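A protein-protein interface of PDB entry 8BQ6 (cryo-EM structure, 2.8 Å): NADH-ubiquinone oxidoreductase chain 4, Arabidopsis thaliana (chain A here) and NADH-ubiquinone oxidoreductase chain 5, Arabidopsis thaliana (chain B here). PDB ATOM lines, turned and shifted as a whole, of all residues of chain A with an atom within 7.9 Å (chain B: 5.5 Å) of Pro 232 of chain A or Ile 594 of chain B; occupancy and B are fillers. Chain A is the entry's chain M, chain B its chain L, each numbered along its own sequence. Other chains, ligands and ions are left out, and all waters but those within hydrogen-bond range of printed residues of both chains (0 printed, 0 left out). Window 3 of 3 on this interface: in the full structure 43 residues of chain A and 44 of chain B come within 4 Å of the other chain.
Printed residues of chain B within 4 Å of His 234 of chain A: Asp 590 (3.1 Å). Of the printed residues of chain B, Ile 235 of chain A touches Ile 594 (3.6 Å) and Pro 599 (3.6 Å). Printed residues of chain B within 4 Å of Tyr 293 of chain A: Leu 589 (3.7 Å). Of the printed residues of chain A, Asp 590 of chain B touches His 234. No residue of chain A comes within 4 Å of Ala 593 of chain B. Ile 594 of chain B touches just these residues of chain A: Pro 232 and Ile 235. Glu 595 of chain B touches none of the printed residues of chain A.
The backbone NH of Ile 594 of chain B is in hydrogen-bond range of the backbone carbonyl oxygen of Leu 589 of chain B (3.0 Å).
Of the 11 printed residues of chain B, 4 touch a printed residue of chain A. Of the 16 printed residues of chain A, 5 touch a printed residue of chain B. Printed residues of chain A that touch a printed residue of chain B: Tyr 176, Pro 232, His 234, Ile 235 and Tyr 293. Among the printed residues, 6 pairs touch across the chains. Among the printed residues, no Asp or Glu carboxylate lies within 4 Å of a Lys or Arg side-chain nitrogen of the other chain.
NE2 of His 234 of chain A sits at hydrogen-bond distance from OD2 of Asp 590 of chain B (3.1 Å).
Among the printed residues, merely in contact across the chains: Tyr 176 of chain A with Pro 599 of chain B (3.6 Å), Pro 232 of chain A with Ile 594 of chain B (3.4 Å), Ile 235 of chain A with Ile 594 of chain B (3.6 Å), Ile 235 of chain A with Pro 599 of chain B (3.6 Å) and Tyr 293 of chain A with Leu 589 of chain B (3.7 Å).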
ATOM      1  N   TYR A 176      23.986 -23.301   4.683  1.00  0.00           N
ATOM      2  CA  TYR A 176      23.243 -22.922   3.483  1.00  0.00           C
ATOM      3  C   TYR A 176      23.467 -21.458   3.130  1.00  0.00           C
ATOM      4  O   TYR A 176      23.769 -21.116   1.972  1.00  0.00           O
ATOM      5  CB  TYR A 176      21.751 -23.170   3.690  1.00  0.00           C
ATOM      6  CG  TYR A 176      21.222 -24.478   3.172  1.00  0.00           C
ATOM      7  CD1 TYR A 176      20.836 -24.614   1.849  1.00  0.00           C
ATOM      8  CD2 TYR A 176      21.051 -25.557   4.020  1.00  0.00           C
ATOM      9  CE1 TYR A 176      20.329 -25.801   1.380  1.00  0.00           C
ATOM     10  CE2 TYR A 176      20.542 -26.745   3.560  1.00  0.00           C
ATOM     11  CZ  TYR A 176      20.184 -26.863   2.241  1.00  0.00           C
ATOM     12  OH  TYR A 176      19.676 -28.053   1.786  1.00  0.00           O
ATOM     13  N   PHE A 221      21.312 -15.701  -8.762  1.00  0.00           N
ATOM     14  CA  PHE A 221      20.226 -16.600  -8.409  1.00  0.00           C
ATOM     15  C   PHE A 221      20.662 -17.617  -7.373  1.00  0.00           C
ATOM     16  O   PHE A 221      19.894 -17.935  -6.464  1.00  0.00           O
ATOM     17  CB  PHE A 221      19.710 -17.317  -9.657  1.00  0.00           C
ATOM     18  CG  PHE A 221      18.715 -18.401  -9.364  1.00  0.00           C
ATOM     19  CD1 PHE A 221      17.406 -18.091  -9.052  1.00  0.00           C
ATOM     20  CD2 PHE A 221      19.093 -19.733  -9.392  1.00  0.00           C
ATOM     21  CE1 PHE A 221      16.493 -19.083  -8.785  1.00  0.00           C
ATOM     22  CE2 PHE A 221      18.181 -20.731  -9.119  1.00  0.00           C
ATOM     23  CZ  PHE A 221      16.879 -20.404  -8.816  1.00  0.00           C
ATOM     24  N   ALA A 225      18.000 -17.380  -4.431  1.00  0.00           N
ATOM     25  CA  ALA A 225      17.073 -18.494  -4.298  1.00  0.00           C
ATOM     26  C   ALA A 225      17.252 -19.217  -2.976  1.00  0.00           C
ATOM     27  O   ALA A 225      16.294 -19.795  -2.454  1.00  0.00           O
ATOM     28  CB  ALA A 225      17.253 -19.469  -5.457  1.00  0.00           C
ATOM     29  N   VAL A 226      18.466 -19.228  -2.428  1.00  0.00           N
ATOM     30  CA  VAL A 226      18.630 -19.779  -1.089  1.00  0.00           C
ATOM     31  C   VAL A 226      18.002 -18.846  -0.066  1.00  0.00           C
ATOM     32  O   VAL A 226      17.400 -19.290   0.919  1.00  0.00           O
ATOM     33  CB  VAL A 226      20.114 -20.048  -0.786  1.00  0.00           C
ATOM     34  CG1 VAL A 226      20.312 -20.263   0.698  1.00  0.00           C
ATOM     35  CG2 VAL A 226      20.588 -21.261  -1.555  1.00  0.00           C
ATOM     36  N   PRO A 229      13.133 -18.606   0.405  1.00  0.00           N
ATOM     37  CA  PRO A 229      13.921 -19.601  -0.324  1.00  0.00           C
ATOM     38  C   PRO A 229      13.116 -20.282  -1.422  1.00  0.00           C
ATOM     39  O   PRO A 229      11.906 -20.454  -1.309  1.00  0.00           O
ATOM     40  CB  PRO A 229      14.303 -20.580   0.784  1.00  0.00           C
ATOM     41  CG  PRO A 229      13.063 -20.624   1.628  1.00  0.00           C
ATOM     42  CD  PRO A 229      12.448 -19.233   1.549  1.00  0.00           C
ATOM     43  N   MET A 230      13.762 -20.696  -2.504  1.00  0.00           N
ATOM     44  CA  MET A 230      13.095 -21.424  -3.567  1.00  0.00           C
ATOM     45  C   MET A 230      13.376 -22.911  -3.413  1.00  0.00           C
ATOM     46  O   MET A 230      14.338 -23.312  -2.755  1.00  0.00           O
ATOM     47  CB  MET A 230      13.547 -20.918  -4.939  1.00  0.00           C
ATOM     48  CG  MET A 230      13.300 -19.431  -5.124  1.00  0.00           C
ATOM     49  SD  MET A 230      13.575 -18.841  -6.799  1.00  0.00           S
ATOM     50  CE  MET A 230      11.950 -19.067  -7.508  1.00  0.00           C
ATOM     51  N   VAL A 231      12.503 -23.731  -3.986  1.00  0.00           N
ATOM     52  CA  VAL A 231      12.723 -25.172  -3.953  1.00  0.00           C
ATOM     53  C   VAL A 231      13.864 -25.482  -4.916  1.00  0.00           C
ATOM     54  O   VAL A 231      14.061 -24.750  -5.897  1.00  0.00           O
ATOM     55  CB  VAL A 231      11.437 -25.943  -4.290  1.00  0.00           C
ATOM     56  CG1 VAL A 231      10.365 -25.628  -3.264  1.00  0.00           C
ATOM     57  CG2 VAL A 231      10.951 -25.595  -5.679  1.00  0.00           C
ATOM     58  N   PRO A 232      14.671 -26.514  -4.659  1.00  0.00           N
ATOM     59  CA  PRO A 232      14.641 -27.423  -3.514  1.00  0.00           C
ATOM     60  C   PRO A 232      15.652 -27.046  -2.435  1.00  0.00           C
ATOM     61  O   PRO A 232      16.164 -27.920  -1.745  1.00  0.00           O
ATOM     62  CB  PRO A 232      14.976 -28.763  -4.167  1.00  0.00           C
ATOM     63  CG  PRO A 232      15.989 -28.385  -5.226  1.00  0.00           C
ATOM     64  CD  PRO A 232      15.654 -26.965  -5.659  1.00  0.00           C
ATOM     65  N   VAL A 233      15.963 -25.762  -2.261  1.00  0.00           N
ATOM     66  CA  VAL A 233      16.966 -25.341  -1.287  1.00  0.00           C
ATOM     67  C   VAL A 233      16.270 -24.595  -0.158  1.00  0.00           C
ATOM     68  O   VAL A 233      16.846 -23.691   0.459  1.00  0.00           O
ATOM     69  CB  VAL A 233      18.057 -24.466  -1.931  1.00  0.00           C
ATOM     70  CG1 VAL A 233      18.904 -25.290  -2.883  1.00  0.00           C
ATOM     71  CG2 VAL A 233      17.447 -23.267  -2.633  1.00  0.00           C
ATOM     72  N   HIS A 234      15.037 -24.994   0.136  1.00  0.00           N
ATOM     73  CA  HIS A 234      14.233 -24.311   1.175  1.00  0.00           C
ATOM     74  C   HIS A 234      14.156 -25.146   2.447  1.00  0.00           C
ATOM     75  O   HIS A 234      13.523 -24.674   3.404  1.00  0.00           O
ATOM     76  CB  HIS A 234      12.812 -24.144   0.636  1.00  0.00           C
ATOM     77  CG  HIS A 234      12.077 -25.436   0.506  1.00  0.00           C
ATOM     78  ND1 HIS A 234      12.459 -26.421  -0.385  1.00  0.00           N
ATOM     79  CD2 HIS A 234      11.002 -25.919   1.161  1.00  0.00           C
ATOM     80  CE1 HIS A 234      11.647 -27.450  -0.277  1.00  0.00           C
ATOM     81  NE2 HIS A 234      10.745 -27.165   0.662  1.00  0.00           N
ATOM     82  N   ILE A 235      14.796 -26.315   2.482  1.00  0.00           N
ATOM     83  CA  ILE A 235      14.576 -27.208   3.613  1.00  0.00           C
ATOM     84  C   ILE A 235      15.283 -26.741   4.879  1.00  0.00           C
ATOM     85  O   ILE A 235      14.982 -27.247   5.965  1.00  0.00           O
ATOM     86  CB  ILE A 235      15.016 -28.643   3.282  1.00  0.00           C
ATOM     87  CG1 ILE A 235      16.509 -28.667   2.971  1.00  0.00           C
ATOM     88  CG2 ILE A 235      14.190 -29.203   2.125  1.00  0.00           C
ATOM     89  CD1 ILE A 235      16.998 -29.974   2.469  1.00  0.00           C
ATOM     90  N   TRP A 236      16.231 -25.808   4.775  1.00  0.00           N
ATOM     91  CA  TRP A 236      16.826 -25.237   5.981  1.00  0.00           C
ATOM     92  C   TRP A 236      15.811 -24.423   6.770  1.00  0.00           C
ATOM     93  O   TRP A 236      15.885 -24.367   8.004  1.00  0.00           O
ATOM     94  CB  TRP A 236      18.028 -24.366   5.614  1.00  0.00           C
ATOM     95  CG  TRP A 236      17.661 -23.211   4.745  1.00  0.00           C
ATOM     96  CD1 TRP A 236      17.636 -23.197   3.385  1.00  0.00           C
ATOM     97  CD2 TRP A 236      17.240 -21.910   5.168  1.00  0.00           C
ATOM     98  NE1 TRP A 236      17.236 -21.967   2.931  1.00  0.00           N
ATOM     99  CE2 TRP A 236      16.986 -21.158   4.007  1.00  0.00           C
ATOM    100  CE3 TRP A 236      17.059 -21.307   6.415  1.00  0.00           C
ATOM    101  CZ2 TRP A 236      16.559 -19.837   4.054  1.00  0.00           C
ATOM    102  CZ3 TRP A 236      16.635 -19.997   6.460  1.00  0.00           C
ATOM    103  CH2 TRP A 236      16.390 -19.275   5.286  1.00  0.00           C
ATOM    104  N   LEU A 286       9.580 -22.567 -11.006  1.00  0.00           N
ATOM    105  CA  LEU A 286      10.029 -22.859  -9.647  1.00  0.00           C
ATOM    106  C   LEU A 286       9.065 -22.290  -8.616  1.00  0.00           C
ATOM    107  O   LEU A 286       8.730 -22.953  -7.629  1.00  0.00           O
ATOM    108  CB  LEU A 286      11.433 -22.298  -9.416  1.00  0.00           C
ATOM    109  CG  LEU A 286      12.658 -23.177  -9.666  1.00  0.00           C
ATOM    110  CD1 LEU A 286      13.897 -22.475  -9.133  1.00  0.00           C
ATOM    111  CD2 LEU A 286      12.510 -24.561  -9.054  1.00  0.00           C
ATOM    112  N   ILE A 289       5.737 -24.342  -8.567  1.00  0.00           N
ATOM    113  CA  ILE A 289       5.915 -25.621  -7.889  1.00  0.00           C
ATOM    114  C   ILE A 289       5.973 -25.418  -6.381  1.00  0.00           C
ATOM    115  O   ILE A 289       5.321 -26.135  -5.615  1.00  0.00           O
ATOM    116  CB  ILE A 289       7.178 -26.327  -8.417  1.00  0.00           C
ATOM    117  CG1 ILE A 289       7.006 -26.721  -9.887  1.00  0.00           C
ATOM    118  CG2 ILE A 289       7.539 -27.524  -7.549  1.00  0.00           C
ATOM    119  CD1 ILE A 289       5.723 -27.437 -10.201  1.00  0.00           C
ATOM    120  N   ALA A 290       6.740 -24.422  -5.934  1.00  0.00           N
ATOM    121  CA  ALA A 290       6.875 -24.175  -4.503  1.00  0.00           C
ATOM    122  C   ALA A 290       5.537 -23.801  -3.883  1.00  0.00           C
ATOM    123  O   ALA A 290       5.218 -24.225  -2.767  1.00  0.00           O
ATOM    124  CB  ALA A 290       7.912 -23.081  -4.254  1.00  0.00           C
ATOM    125  N   TYR A 293       3.348 -27.215  -4.008  1.00  0.00           N
ATOM    126  CA  TYR A 293       3.879 -28.335  -3.237  1.00  0.00           C
ATOM    127  C   TYR A 293       3.980 -28.000  -1.756  1.00  0.00           C
ATOM    128  O   TYR A 293       3.556 -28.788  -0.902  1.00  0.00           O
ATOM    129  CB  TYR A 293       5.246 -28.747  -3.771  1.00  0.00           C
ATOM    130  CG  TYR A 293       5.230 -29.621  -4.999  1.00  0.00           C
ATOM    131  CD1 TYR A 293       4.151 -29.633  -5.875  1.00  0.00           C
ATOM    132  CD2 TYR A 293       6.302 -30.450  -5.272  1.00  0.00           C
ATOM    133  CE1 TYR A 293       4.160 -30.441  -6.994  1.00  0.00           C
ATOM    134  CE2 TYR A 293       6.318 -31.252  -6.372  1.00  0.00           C
ATOM    135  CZ  TYR A 293       5.253 -31.249  -7.231  1.00  0.00           C
ATOM    136  OH  TYR A 293       5.300 -32.070  -8.326  1.00  0.00           O
ATOM    137  N   ALA B 588       8.638 -38.067   0.306  1.00  0.00           N
ATOM    138  CA  ALA B 588       9.449 -38.486  -0.832  1.00  0.00           C
ATOM    139  C   ALA B 588      10.403 -37.385  -1.279  1.00  0.00           C
ATOM    140  O   ALA B 588      11.549 -37.666  -1.649  1.00  0.00           O
ATOM    141  CB  ALA B 588       8.552 -38.918  -1.990  1.00  0.00           C
ATOM    142  N   LEU B 589       9.949 -36.132  -1.276  1.00  0.00           N
ATOM    143  CA  LEU B 589      10.792 -35.042  -1.751  1.00  0.00           C
ATOM    144  C   LEU B 589      11.498 -34.305  -0.617  1.00  0.00           C
ATOM    145  O   LEU B 589      12.729 -34.340  -0.535  1.00  0.00           O
ATOM    146  CB  LEU B 589       9.963 -34.066  -2.586  1.00  0.00           C
ATOM    147  CG  LEU B 589       9.524 -34.572  -3.964  1.00  0.00           C
ATOM    148  CD1 LEU B 589       8.524 -33.625  -4.592  1.00  0.00           C
ATOM    149  CD2 LEU B 589      10.726 -34.744  -4.877  1.00  0.00           C
ATOM    150  N   ASP B 590      10.754 -33.580   0.225  1.00  0.00           N
ATOM    151  CA  ASP B 590      11.418 -32.729   1.258  1.00  0.00           C
ATOM    152  C   ASP B 590      12.274 -33.588   2.194  1.00  0.00           C
ATOM    153  O   ASP B 590      13.459 -33.267   2.361  1.00  0.00           O
ATOM    154  CB  ASP B 590      10.424 -31.870   2.039  1.00  0.00           C
ATOM    155  CG  ASP B 590      10.014 -30.598   1.319  1.00  0.00           C
ATOM    156  OD1 ASP B 590      10.189 -30.532   0.086  1.00  0.00           O
ATOM    157  OD2 ASP B 590       9.511 -29.686   1.995  1.00  0.00           O
ATOM    158  N   GLY B 592      12.943 -36.761   1.722  1.00  0.00           N
ATOM    159  CA  GLY B 592      13.464 -37.891   0.990  1.00  0.00           C
ATOM    160  C   GLY B 592      14.661 -37.526   0.140  1.00  0.00           C
ATOM    161  O   GLY B 592      15.774 -37.355   0.648  1.00  0.00           O
ATOM    162  N   ALA B 593      14.422 -37.393  -1.165  1.00  0.00           N
ATOM    163  CA  ALA B 593      15.504 -37.183  -2.123  1.00  0.00           C
ATOM    164  C   ALA B 593      16.257 -35.884  -1.862  1.00  0.00           C
ATOM    165  O   ALA B 593      17.485 -35.837  -2.002  1.00  0.00           O
ATOM    166  CB  ALA B 593      14.945 -37.192  -3.543  1.00  0.00           C
ATOM    167  N   ILE B 594      15.542 -34.809  -1.523  1.00  0.00           N
ATOM    168  CA  ILE B 594      16.208 -33.535  -1.265  1.00  0.00           C
ATOM    169  C   ILE B 594      17.136 -33.651  -0.065  1.00  0.00           C
ATOM    170  O   ILE B 594      18.228 -33.072  -0.049  1.00  0.00           O
ATOM    171  CB  ILE B 594      15.178 -32.411  -1.075  1.00  0.00           C
ATOM    172  CG1 ILE B 594      14.311 -32.257  -2.322  1.00  0.00           C
ATOM    173  CG2 ILE B 594      15.865 -31.102  -0.733  1.00  0.00           C
ATOM    174  CD1 ILE B 594      13.247 -31.213  -2.164  1.00  0.00           C
ATOM    175  N   GLU B 595      16.712 -34.384   0.965  1.00  0.00           N
ATOM    176  CA  GLU B 595      17.589 -34.618   2.106  1.00  0.00           C
ATOM    177  C   GLU B 595      18.778 -35.489   1.724  1.00  0.00           C
ATOM    178  O   GLU B 595      19.919 -35.184   2.089  1.00  0.00           O
ATOM    179  CB  GLU B 595      16.811 -35.266   3.249  1.00  0.00           C
ATOM    180  CG  GLU B 595      16.204 -34.290   4.236  1.00  0.00           C
ATOM    181  CD  GLU B 595      17.240 -33.508   5.022  1.00  0.00           C
ATOM    182  OE1 GLU B 595      18.439 -33.849   4.971  1.00  0.00           O
ATOM    183  OE2 GLU B 595      16.851 -32.536   5.700  1.00  0.00           O
ATOM    184  N   ILE B 596      18.531 -36.587   1.008  1.00  0.00           N
ATOM    185  CA  ILE B 596      19.621 -37.483   0.632  1.00  0.00           C
ATOM    186  C   ILE B 596      20.582 -36.784  -0.321  1.00  0.00           C
ATOM    187  O   ILE B 596      21.805 -36.857  -0.151  1.00  0.00           O
ATOM    188  CB  ILE B 596      19.065 -38.793   0.042  1.00  0.00           C
ATOM    189  CG1 ILE B 596      18.992 -39.879   1.118  1.00  0.00           C
ATOM    190  CG2 ILE B 596      19.924 -39.288  -1.104  1.00  0.00           C
ATOM    191  CD1 ILE B 596      18.331 -39.451   2.400  1.00  0.00           C
ATOM    192  N   LEU B 597      20.057 -36.080  -1.319  1.00  0.00           N
ATOM    193  CA  LEU B 597      20.911 -35.286  -2.201  1.00  0.00           C
ATOM    194  C   LEU B 597      21.064 -33.867  -1.669  1.00  0.00           C
ATOM    195  O   LEU B 597      20.919 -32.879  -2.386  1.00  0.00           O
ATOM    196  CB  LEU B 597      20.348 -35.282  -3.616  1.00  0.00           C
ATOM    197  CG  LEU B 597      20.107 -36.637  -4.283  1.00  0.00           C
ATOM    198  CD1 LEU B 597      19.824 -36.439  -5.758  1.00  0.00           C
ATOM    199  CD2 LEU B 597      21.290 -37.568  -4.087  1.00  0.00           C
ATOM    200  N   GLY B 598      21.395 -33.775  -0.389  1.00  0.00           N
ATOM    201  CA  GLY B 598      21.516 -32.513   0.291  1.00  0.00           C
ATOM    202  C   GLY B 598      22.149 -32.713   1.649  1.00  0.00           C
ATOM    203  O   GLY B 598      23.075 -33.511   1.811  1.00  0.00           O
ATOM    204  N   PRO B 599      21.621 -32.028   2.666  1.00  0.00           N
ATOM    205  CA  PRO B 599      22.314 -31.998   3.968  1.00  0.00           C
ATOM    206  C   PRO B 599      22.561 -33.366   4.579  1.00  0.00           C
ATOM    207  O   PRO B 599      23.627 -33.588   5.167  1.00  0.00           O
ATOM    208  CB  PRO B 599      21.384 -31.156   4.854  1.00  0.00           C
ATOM    209  CG  PRO B 599      20.220 -30.765   4.021  1.00  0.00           C
ATOM    210  CD  PRO B 599      20.252 -31.496   2.728  1.00  0.00           C
